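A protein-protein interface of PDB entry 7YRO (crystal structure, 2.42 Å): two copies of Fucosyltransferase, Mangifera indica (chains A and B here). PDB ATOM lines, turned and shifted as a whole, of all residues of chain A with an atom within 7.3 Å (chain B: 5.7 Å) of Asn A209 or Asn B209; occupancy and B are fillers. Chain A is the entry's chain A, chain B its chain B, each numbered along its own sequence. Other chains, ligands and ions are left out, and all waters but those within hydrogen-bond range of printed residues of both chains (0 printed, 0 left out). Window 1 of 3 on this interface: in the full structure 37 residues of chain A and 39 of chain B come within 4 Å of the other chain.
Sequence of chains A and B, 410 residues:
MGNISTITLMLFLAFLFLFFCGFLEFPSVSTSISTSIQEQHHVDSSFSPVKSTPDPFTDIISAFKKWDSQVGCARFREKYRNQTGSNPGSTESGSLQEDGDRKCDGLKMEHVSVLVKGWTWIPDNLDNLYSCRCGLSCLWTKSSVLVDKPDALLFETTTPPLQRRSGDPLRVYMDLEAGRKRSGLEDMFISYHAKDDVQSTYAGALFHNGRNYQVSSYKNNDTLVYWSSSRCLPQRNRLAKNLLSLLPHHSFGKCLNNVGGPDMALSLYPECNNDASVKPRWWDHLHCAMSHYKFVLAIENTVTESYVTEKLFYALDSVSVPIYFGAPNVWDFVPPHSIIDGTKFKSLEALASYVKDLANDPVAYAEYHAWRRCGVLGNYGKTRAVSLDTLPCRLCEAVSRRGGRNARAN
The side-chain amide nitrogen of Asn A125 lies close to the side-chain amide nitrogen of Asn B209 (3.3 Å). ND2 of Asn A209 lies close to ND2 of Asn B209, 2.9 Å away.
OD1 of Asn A209 is in hydrogen-bond range of OH of Tyr A213, at 2.7 Å. ND2 of Asn B125 sits at hydrogen-bond distance from O of Leu B206 (2.7 Å). The backbone carbonyl oxygen of Asn B209 is in hydrogen-bond range of the side-chain hydroxyl of Tyr B213.
Among the printed residues, pairs that only touch across the chains: Asn A209 with Asn B125 (3.2 Å), Tyr A213 with Asn B125 (3.4 Å), Asp A124 with Tyr B213 (3.5 Å), Asp A127 with Tyr B213 (3.8 Å) and Asn A125 with Tyr B213 (3.96 Å).
Asn A209 touches just these residues of chain B: Asn B125 (3.2 Å) and Asn B209 (2.9 Å). Asn B209 touches two residues of chain A. Of the printed residues of chain B, Asn A125 touches Asn B209 (3.2 Å) and Tyr B213 (3.96 Å). Printed residues of chain B within 4 Å of Asp A127: Tyr B213 (3.8 Å). Gly A210 touches none of the printed residues of chain B. The nearest residue of chain A that does not touch Asn B209 is Leu A206 (4.5 Å). The nearest printed residue of chain B that does not touch Asn A125 is Gly B210 (4.7 Å).
Of the 17 printed residues of chain A, 5 touch a printed residue of chain B. Printed residues of chain A that touch a printed residue of chain B: Asp A124, Asn A125, Asp A127, Asn A209 and Tyr A213. Hydrophobic or aromatic side chains of chain A that line the printed part of chain B: Tyr A213. Of the 10 printed residues of chain B, 3 touch a printed residue of chain A. Hydrophobic or aromatic side chains of chain B that line the printed part of chain A: Tyr B213. Among the printed residues, 7 pairs touch across the chains. Among the printed residues, no Asp or Glu carboxylate lies within 4 Å of a Lys or Arg side-chain nitrogen of the other chain.
Asn A125 touches Asn B209, and with the chains exchanged Asn A209 touches Asn B125. Asn A125 touches Tyr B213, and with the chains exchanged Tyr A213 touches Asn B125. Asn B209 touches its own counterpart, Asn A209. Positions printed for both chains: 125, 205, 206, 207, 208, 209, 210, 211, 213 and 283.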
ATOM      1  N   PRO A 123      -7.518 -26.375 -17.691  1.00  0.00           N
ATOM      2  CA  PRO A 123      -6.772 -26.781 -18.885  1.00  0.00           C
ATOM      3  C   PRO A 123      -5.992 -28.071 -18.692  1.00  0.00           C
ATOM      4  O   PRO A 123      -5.561 -28.420 -17.589  1.00  0.00           O
ATOM      5  CB  PRO A 123      -5.816 -25.603 -19.125  1.00  0.00           C
ATOM      6  CG  PRO A 123      -6.246 -24.518 -18.173  1.00  0.00           C
ATOM      7  CD  PRO A 123      -6.920 -25.201 -17.038  1.00  0.00           C
ATOM      8  N   ASP A 124      -5.813 -28.786 -19.804  1.00  0.00           N
ATOM      9  CA  ASP A 124      -4.970 -29.976 -19.784  1.00  0.00           C
ATOM     10  C   ASP A 124      -3.528 -29.614 -19.462  1.00  0.00           C
ATOM     11  O   ASP A 124      -2.806 -30.417 -18.854  1.00  0.00           O
ATOM     12  CB  ASP A 124      -5.053 -30.723 -21.114  1.00  0.00           C
ATOM     13  CG  ASP A 124      -6.407 -31.371 -21.335  1.00  0.00           C
ATOM     14  OD1 ASP A 124      -7.133 -31.576 -20.341  1.00  0.00           O
ATOM     15  OD2 ASP A 124      -6.740 -31.687 -22.498  1.00  0.00           O
ATOM     16  N   ASN A 125      -3.091 -28.413 -19.855  1.00  0.00           N
ATOM     17  CA  ASN A 125      -1.699 -28.016 -19.688  1.00  0.00           C
ATOM     18  C   ASN A 125      -1.308 -27.823 -18.235  1.00  0.00           C
ATOM     19  O   ASN A 125      -0.145 -27.502 -17.971  1.00  0.00           O
ATOM     20  CB  ASN A 125      -1.445 -26.696 -20.409  1.00  0.00           C
ATOM     21  CG  ASN A 125      -1.925 -26.706 -21.837  1.00  0.00           C
ATOM     22  OD1 ASN A 125      -2.172 -27.763 -22.420  1.00  0.00           O
ATOM     23  ND2 ASN A 125      -2.080 -25.516 -22.411  1.00  0.00           N
ATOM     24  N   LEU A 126      -2.229 -28.007 -17.288  1.00  0.00           N
ATOM     25  CA  LEU A 126      -1.846 -28.097 -15.889  1.00  0.00           C
ATOM     26  C   LEU A 126      -1.340 -29.477 -15.502  1.00  0.00           C
ATOM     27  O   LEU A 126      -0.633 -29.594 -14.496  1.00  0.00           O
ATOM     28  CB  LEU A 126      -3.027 -27.722 -14.995  1.00  0.00           C
ATOM     29  CG  LEU A 126      -3.211 -26.235 -14.701  1.00  0.00           C
ATOM     30  CD1 LEU A 126      -4.376 -26.043 -13.749  1.00  0.00           C
ATOM     31  CD2 LEU A 126      -1.939 -25.623 -14.145  1.00  0.00           C
ATOM     32  N   ASP A 127      -1.681 -30.517 -16.267  1.00  0.00           N
ATOM     33  CA  ASP A 127      -1.274 -31.869 -15.900  1.00  0.00           C
ATOM     34  C   ASP A 127       0.243 -31.976 -15.917  1.00  0.00           C
ATOM     35  O   ASP A 127       0.882 -31.699 -16.936  1.00  0.00           O
ATOM     36  CB  ASP A 127      -1.888 -32.896 -16.852  1.00  0.00           C
ATOM     37  CG  ASP A 127      -3.376 -33.101 -16.618  1.00  0.00           C
ATOM     38  OD1 ASP A 127      -3.986 -32.283 -15.899  1.00  0.00           O
ATOM     39  OD2 ASP A 127      -3.931 -34.091 -17.143  1.00  0.00           O
ATOM     40  N   ALA A 205      -0.170 -17.512 -16.861  1.00  0.00           N
ATOM     41  CA  ALA A 205       0.091 -17.776 -18.265  1.00  0.00           C
ATOM     42  C   ALA A 205      -0.386 -19.145 -18.721  1.00  0.00           C
ATOM     43  O   ALA A 205      -0.383 -19.407 -19.927  1.00  0.00           O
ATOM     44  CB  ALA A 205       1.591 -17.641 -18.566  1.00  0.00           C
ATOM     45  N   LEU A 206      -0.799 -20.021 -17.799  1.00  0.00           N
ATOM     46  CA  LEU A 206      -1.094 -21.399 -18.182  1.00  0.00           C
ATOM     47  C   LEU A 206      -2.461 -21.539 -18.841  1.00  0.00           C
ATOM     48  O   LEU A 206      -2.592 -22.281 -19.820  1.00  0.00           O
ATOM     49  CB  LEU A 206      -0.973 -22.331 -16.978  1.00  0.00           C
ATOM     50  CG  LEU A 206       0.364 -23.071 -16.912  1.00  0.00           C
ATOM     51  CD1 LEU A 206       0.437 -24.076 -18.052  1.00  0.00           C
ATOM     52  CD2 LEU A 206       1.543 -22.113 -16.972  1.00  0.00           C
ATOM     53  N   PHE A 207      -3.497 -20.868 -18.337  1.00  0.00           N
ATOM     54  CA  PHE A 207      -4.744 -20.824 -19.089  1.00  0.00           C
ATOM     55  C   PHE A 207      -4.577 -19.899 -20.287  1.00  0.00           C
ATOM     56  O   PHE A 207      -3.996 -18.812 -20.173  1.00  0.00           O
ATOM     57  CB  PHE A 207      -5.956 -20.416 -18.223  1.00  0.00           C
ATOM     58  CG  PHE A 207      -5.718 -19.312 -17.195  1.00  0.00           C
ATOM     59  CD1 PHE A 207      -4.621 -18.467 -17.230  1.00  0.00           C
ATOM     60  CD2 PHE A 207      -6.651 -19.129 -16.178  1.00  0.00           C
ATOM     61  CE1 PHE A 207      -4.455 -17.480 -16.267  1.00  0.00           C
ATOM     62  CE2 PHE A 207      -6.489 -18.148 -15.220  1.00  0.00           C
ATOM     63  CZ  PHE A 207      -5.394 -17.323 -15.265  1.00  0.00           C
ATOM     64  N   HIS A 208      -5.071 -20.352 -21.440  1.00  0.00           N
ATOM     65  CA  HIS A 208      -4.877 -19.725 -22.744  1.00  0.00           C
ATOM     66  C   HIS A 208      -3.433 -19.809 -23.214  1.00  0.00           C
ATOM     67  O   HIS A 208      -2.985 -18.982 -24.014  1.00  0.00           O
ATOM     68  CB  HIS A 208      -5.379 -18.281 -22.764  1.00  0.00           C
ATOM     69  CG  HIS A 208      -6.831 -18.168 -22.434  1.00  0.00           C
ATOM     70  ND1 HIS A 208      -7.292 -17.508 -21.317  1.00  0.00           N
ATOM     71  CD2 HIS A 208      -7.922 -18.686 -23.045  1.00  0.00           C
ATOM     72  CE1 HIS A 208      -8.610 -17.588 -21.276  1.00  0.00           C
ATOM     73  NE2 HIS A 208      -9.017 -18.300 -22.313  1.00  0.00           N
ATOM     74  N   ASN A 209      -2.684 -20.778 -22.699  1.00  0.00           N
ATOM     75  CA  ASN A 209      -1.348 -21.029 -23.209  1.00  0.00           C
ATOM     76  C   ASN A 209      -1.471 -21.604 -24.617  1.00  0.00           C
ATOM     77  O   ASN A 209      -2.404 -22.351 -24.926  1.00  0.00           O
ATOM     78  CB  ASN A 209      -0.590 -21.993 -22.298  1.00  0.00           C
ATOM     79  CG  ASN A 209       0.911 -21.901 -22.472  1.00  0.00           C
ATOM     80  OD1 ASN A 209       1.432 -20.878 -22.916  1.00  0.00           O
ATOM     81  ND2 ASN A 209       1.615 -22.969 -22.116  1.00  0.00           N
ATOM     82  N   GLY A 210      -0.523 -21.256 -25.474  1.00  0.00           N
ATOM     83  CA  GLY A 210      -0.620 -21.720 -26.842  1.00  0.00           C
ATOM     84  C   GLY A 210      -1.379 -20.702 -27.665  1.00  0.00           C
ATOM     85  O   GLY A 210      -2.369 -21.013 -28.334  1.00  0.00           O
ATOM     86  N   ARG A 211      -0.909 -19.467 -27.590  1.00  0.00           N
ATOM     87  CA  ARG A 211      -1.467 -18.286 -28.224  1.00  0.00           C
ATOM     88  C   ARG A 211      -0.435 -17.697 -29.179  1.00  0.00           C
ATOM     89  O   ARG A 211       0.665 -18.223 -29.342  1.00  0.00           O
ATOM     90  CB  ARG A 211      -1.846 -17.251 -27.164  1.00  0.00           C
ATOM     91  CG  ARG A 211      -0.610 -16.727 -26.444  1.00  0.00           C
ATOM     92  CD  ARG A 211      -0.897 -15.645 -25.425  1.00  0.00           C
ATOM     93  NE  ARG A 211       0.208 -14.696 -25.364  1.00  0.00           N
ATOM     94  CZ  ARG A 211       0.618 -14.088 -24.261  1.00  0.00           C
ATOM     95  NH1 ARG A 211       0.060 -14.335 -23.087  1.00  0.00           N
ATOM     96  NH2 ARG A 211       1.619 -13.215 -24.334  1.00  0.00           N
ATOM     97  N   ASN A 212      -0.777 -16.562 -29.778  1.00  0.00           N
ATOM     98  CA  ASN A 212       0.192 -15.804 -30.558  1.00  0.00           C
ATOM     99  C   ASN A 212       0.934 -14.864 -29.616  1.00  0.00           C
ATOM    100  O   ASN A 212       0.310 -14.139 -28.833  1.00  0.00           O
ATOM    101  CB  ASN A 212      -0.488 -15.016 -31.678  1.00  0.00           C
ATOM    102  CG  ASN A 212       0.501 -14.222 -32.518  1.00  0.00           C
ATOM    103  OD1 ASN A 212       1.126 -13.275 -32.041  1.00  0.00           O
ATOM    104  ND2 ASN A 212       0.634 -14.599 -33.785  1.00  0.00           N
ATOM    105  N   TYR A 213       2.261 -14.862 -29.702  1.00  0.00           N
ATOM    106  CA  TYR A 213       3.079 -14.101 -28.769  1.00  0.00           C
ATOM    107  C   TYR A 213       3.682 -12.856 -29.400  1.00  0.00           C
ATOM    108  O   TYR A 213       4.533 -12.210 -28.780  1.00  0.00           O
ATOM    109  CB  TYR A 213       4.183 -14.982 -28.185  1.00  0.00           C
ATOM    110  CG  TYR A 213       3.690 -15.999 -27.178  1.00  0.00           C
ATOM    111  CD1 TYR A 213       3.139 -17.207 -27.586  1.00  0.00           C
ATOM    112  CD2 TYR A 213       3.767 -15.746 -25.815  1.00  0.00           C
ATOM    113  CE1 TYR A 213       2.685 -18.140 -26.662  1.00  0.00           C
ATOM    114  CE2 TYR A 213       3.315 -16.672 -24.885  1.00  0.00           C
ATOM    115  CZ  TYR A 213       2.775 -17.866 -25.315  1.00  0.00           C
ATOM    116  OH  TYR A 213       2.324 -18.786 -24.399  1.00  0.00           O
ATOM    117  N   ASN A 274      -2.780 -17.505 -35.404  1.00  0.00           N
ATOM    118  CA  ASN A 274      -2.146 -18.646 -34.754  1.00  0.00           C
ATOM    119  C   ASN A 274      -2.099 -19.817 -35.728  1.00  0.00           C
ATOM    120  O   ASN A 274      -3.140 -20.253 -36.231  1.00  0.00           O
ATOM    121  CB  ASN A 274      -2.904 -19.035 -33.484  1.00  0.00           C
ATOM    122  CG  ASN A 274      -2.028 -19.757 -32.478  1.00  0.00           C
ATOM    123  OD1 ASN A 274      -0.800 -19.669 -32.528  1.00  0.00           O
ATOM    124  ND2 ASN A 274      -2.656 -20.483 -31.558  1.00  0.00           N
ATOM    125  N   TRP A 283      -9.154 -16.272 -28.069  1.00  0.00           N
ATOM    126  CA  TRP A 283      -8.027 -15.897 -27.226  1.00  0.00           C
ATOM    127  C   TRP A 283      -6.660 -16.111 -27.867  1.00  0.00           C
ATOM    128  O   TRP A 283      -5.658 -15.666 -27.296  1.00  0.00           O
ATOM    129  CB  TRP A 283      -8.096 -16.683 -25.913  1.00  0.00           C
ATOM    130  CG  TRP A 283      -8.284 -18.155 -26.146  1.00  0.00           C
ATOM    131  CD1 TRP A 283      -9.468 -18.834 -26.132  1.00  0.00           C
ATOM    132  CD2 TRP A 283      -7.275 -19.118 -26.474  1.00  0.00           C
ATOM    133  NE1 TRP A 283      -9.257 -20.163 -26.407  1.00  0.00           N
ATOM    134  CE2 TRP A 283      -7.920 -20.364 -26.624  1.00  0.00           C
ATOM    135  CE3 TRP A 283      -5.889 -19.053 -26.645  1.00  0.00           C
ATOM    136  CZ2 TRP A 283      -7.228 -21.532 -26.938  1.00  0.00           C
ATOM    137  CZ3 TRP A 283      -5.202 -20.216 -26.957  1.00  0.00           C
ATOM    138  CH2 TRP A 283      -5.873 -21.437 -27.098  1.00  0.00           C
ATOM    139  N   TYR A 314      -4.006  -9.383 -19.247  1.00  0.00           N
ATOM    140  CA  TYR A 314      -3.558  -9.589 -20.622  1.00  0.00           C
ATOM    141  C   TYR A 314      -3.067  -8.284 -21.244  1.00  0.00           C
ATOM    142  O   TYR A 314      -2.102  -8.279 -22.022  1.00  0.00           O
ATOM    143  CB  TYR A 314      -4.679 -10.210 -21.454  1.00  0.00           C
ATOM    144  CG  TYR A 314      -4.916 -11.671 -21.137  1.00  0.00           C
ATOM    145  CD1 TYR A 314      -4.143 -12.327 -20.186  1.00  0.00           C
ATOM    146  CD2 TYR A 314      -5.902 -12.398 -21.792  1.00  0.00           C
ATOM    147  CE1 TYR A 314      -4.348 -13.662 -19.886  1.00  0.00           C
ATOM    148  CE2 TYR A 314      -6.115 -13.740 -21.502  1.00  0.00           C
ATOM    149  CZ  TYR A 314      -5.332 -14.365 -20.546  1.00  0.00           C
ATOM    150  OH  TYR A 314      -5.529 -15.692 -20.240  1.00  0.00           O
ATOM    151  N   ASN B 125       5.712 -20.829 -25.590  1.00  0.00           N
ATOM    152  CA  ASN B 125       4.985 -20.909 -24.322  1.00  0.00           C
ATOM    153  C   ASN B 125       5.900 -20.949 -23.100  1.00  0.00           C
ATOM    154  O   ASN B 125       5.388 -21.151 -21.993  1.00  0.00           O
ATOM    155  CB  ASN B 125       4.038 -22.111 -24.318  1.00  0.00           C
ATOM    156  CG  ASN B 125       4.690 -23.366 -24.829  1.00  0.00           C
ATOM    157  OD1 ASN B 125       5.120 -23.427 -25.981  1.00  0.00           O
ATOM    158  ND2 ASN B 125       4.768 -24.381 -23.979  1.00  0.00           N
ATOM    159  N   ALA B 205       7.402 -30.821 -18.899  1.00  0.00           N
ATOM    160  CA  ALA B 205       6.111 -30.943 -19.558  1.00  0.00           C
ATOM    161  C   ALA B 205       5.778 -29.787 -20.488  1.00  0.00           C
ATOM    162  O   ALA B 205       4.801 -29.883 -21.237  1.00  0.00           O
ATOM    163  CB  ALA B 205       4.994 -31.081 -18.514  1.00  0.00           C
ATOM    164  N   LEU B 206       6.554 -28.701 -20.466  1.00  0.00           N
ATOM    165  CA  LEU B 206       6.163 -27.500 -21.199  1.00  0.00           C
ATOM    166  C   LEU B 206       6.479 -27.551 -22.688  1.00  0.00           C
ATOM    167  O   LEU B 206       5.821 -26.837 -23.456  1.00  0.00           O
ATOM    168  CB  LEU B 206       6.828 -26.260 -20.595  1.00  0.00           C
ATOM    169  CG  LEU B 206       5.982 -25.439 -19.620  1.00  0.00           C
ATOM    170  CD1 LEU B 206       6.791 -24.301 -19.016  1.00  0.00           C
ATOM    171  CD2 LEU B 206       4.742 -24.901 -20.314  1.00  0.00           C
ATOM    172  N   PHE B 207       7.452 -28.360 -23.119  1.00  0.00           N
ATOM    173  CA  PHE B 207       7.920 -28.271 -24.499  1.00  0.00           C
ATOM    174  C   PHE B 207       6.798 -28.523 -25.502  1.00  0.00           C
ATOM    175  O   PHE B 207       6.401 -27.608 -26.231  1.00  0.00           O
ATOM    176  CB  PHE B 207       9.069 -29.246 -24.750  1.00  0.00           C
ATOM    177  CG  PHE B 207       9.606 -29.190 -26.152  1.00  0.00           C
ATOM    178  CD1 PHE B 207       9.536 -28.016 -26.891  1.00  0.00           C
ATOM    179  CD2 PHE B 207      10.159 -30.312 -26.743  1.00  0.00           C
ATOM    180  CE1 PHE B 207      10.013 -27.962 -28.185  1.00  0.00           C
ATOM    181  CE2 PHE B 207      10.644 -30.263 -28.039  1.00  0.00           C
ATOM    182  CZ  PHE B 207      10.569 -29.084 -28.760  1.00  0.00           C
ATOM    183  N   HIS B 208       6.279 -29.748 -25.558  1.00  0.00           N
ATOM    184  CA  HIS B 208       5.090 -30.036 -26.360  1.00  0.00           C
ATOM    185  C   HIS B 208       3.897 -30.089 -25.414  1.00  0.00           C
ATOM    186  O   HIS B 208       3.399 -31.147 -25.025  1.00  0.00           O
ATOM    187  CB  HIS B 208       5.271 -31.304 -27.186  1.00  0.00           C
ATOM    188  CG  HIS B 208       6.361 -31.199 -28.209  1.00  0.00           C
ATOM    189  ND1 HIS B 208       6.388 -30.199 -29.159  1.00  0.00           N
ATOM    190  CD2 HIS B 208       7.449 -31.971 -28.447  1.00  0.00           C
ATOM    191  CE1 HIS B 208       7.448 -30.352 -29.930  1.00  0.00           C
ATOM    192  NE2 HIS B 208       8.107 -31.422 -29.521  1.00  0.00           N
ATOM    193  N   ASN B 209       3.444 -28.891 -25.051  1.00  0.00           N
ATOM    194  CA  ASN B 209       2.344 -28.723 -24.112  1.00  0.00           C
ATOM    195  C   ASN B 209       1.024 -29.198 -24.722  1.00  0.00           C
ATOM    196  O   ASN B 209       0.266 -29.945 -24.090  1.00  0.00           O
ATOM    197  CB  ASN B 209       2.292 -27.246 -23.710  1.00  0.00           C
ATOM    198  CG  ASN B 209       1.685 -27.026 -22.353  1.00  0.00           C
ATOM    199  OD1 ASN B 209       1.734 -27.902 -21.490  1.00  0.00           O
ATOM    200  ND2 ASN B 209       1.155 -25.830 -22.132  1.00  0.00           N
ATOM    201  N   GLY B 210       0.727 -28.761 -25.947  1.00  0.00           N
ATOM    202  CA  GLY B 210      -0.477 -29.143 -26.663  1.00  0.00           C
ATOM    203  C   GLY B 210      -0.546 -30.575 -27.160  1.00  0.00           C
ATOM    204  O   GLY B 210      -0.466 -30.805 -28.370  1.00  0.00           O
ATOM    205  N   ARG B 211      -0.696 -31.549 -26.264  1.00  0.00           N
ATOM    206  CA  ARG B 211      -0.733 -32.956 -26.650  1.00  0.00           C
ATOM    207  C   ARG B 211      -2.006 -33.610 -26.117  1.00  0.00           C
ATOM    208  O   ARG B 211      -2.810 -32.985 -25.422  1.00  0.00           O
ATOM    209  CB  ARG B 211       0.515 -33.698 -26.150  1.00  0.00           C
ATOM    210  CG  ARG B 211       0.821 -33.495 -24.675  1.00  0.00           C
ATOM    211  CD  ARG B 211       1.112 -34.819 -23.992  1.00  0.00           C
ATOM    212  NE  ARG B 211       1.563 -34.645 -22.617  1.00  0.00           N
ATOM    213  CZ  ARG B 211       1.432 -35.563 -21.671  1.00  0.00           C
ATOM    214  NH1 ARG B 211       0.833 -36.716 -21.907  1.00  0.00           N
ATOM    215  NH2 ARG B 211       1.907 -35.313 -20.454  1.00  0.00           N
ATOM    216  N   TYR B 213      -3.807 -36.163 -23.628  1.00  0.00           N
ATOM    217  CA  TYR B 213      -3.522 -36.582 -22.262  1.00  0.00           C
ATOM    218  C   TYR B 213      -4.238 -37.867 -21.868  1.00  0.00           C
ATOM    219  O   TYR B 213      -4.220 -38.236 -20.687  1.00  0.00           O
ATOM    220  CB  TYR B 213      -3.873 -35.454 -21.289  1.00  0.00           C
ATOM    221  CG  TYR B 213      -2.897 -34.304 -21.356  1.00  0.00           C
ATOM    222  CD1 TYR B 213      -3.010 -33.331 -22.339  1.00  0.00           C
ATOM    223  CD2 TYR B 213      -1.847 -34.204 -20.454  1.00  0.00           C
ATOM    224  CE1 TYR B 213      -2.114 -32.283 -22.413  1.00  0.00           C
ATOM    225  CE2 TYR B 213      -0.944 -33.157 -20.521  1.00  0.00           C
ATOM    226  CZ  TYR B 213      -1.082 -32.200 -21.503  1.00  0.00           C
ATOM    227  OH  TYR B 213      -0.185 -31.155 -21.575  1.00  0.00           O
ATOM    228  N   TRP B 283       3.726 -34.857 -32.693  1.00  0.00           N
ATOM    229  CA  TRP B 283       3.941 -35.164 -31.280  1.00  0.00           C
ATOM    230  C   TRP B 283       2.650 -35.242 -30.470  1.00  0.00           C
ATOM    231  O   TRP B 283       2.712 -35.511 -29.266  1.00  0.00           O
ATOM    232  CB  TRP B 283       4.845 -34.123 -30.617  1.00  0.00           C
ATOM    233  CG  TRP B 283       4.283 -32.738 -30.651  1.00  0.00           C
ATOM    234  CD1 TRP B 283       3.370 -32.213 -29.781  1.00  0.00           C
ATOM    235  CD2 TRP B 283       4.596 -31.692 -31.577  1.00  0.00           C
ATOM    236  NE1 TRP B 283       3.088 -30.913 -30.111  1.00  0.00           N
ATOM    237  CE2 TRP B 283       3.829 -30.567 -31.210  1.00  0.00           C
ATOM    238  CE3 TRP B 283       5.446 -31.597 -32.680  1.00  0.00           C
ATOM    239  CZ2 TRP B 283       3.887 -29.363 -31.908  1.00  0.00           C
ATOM    240  CZ3 TRP B 283       5.502 -30.397 -33.374  1.00  0.00           C
ATOM    241  CH2 TRP B 283       4.728 -29.298 -32.985  1.00  0.00           C
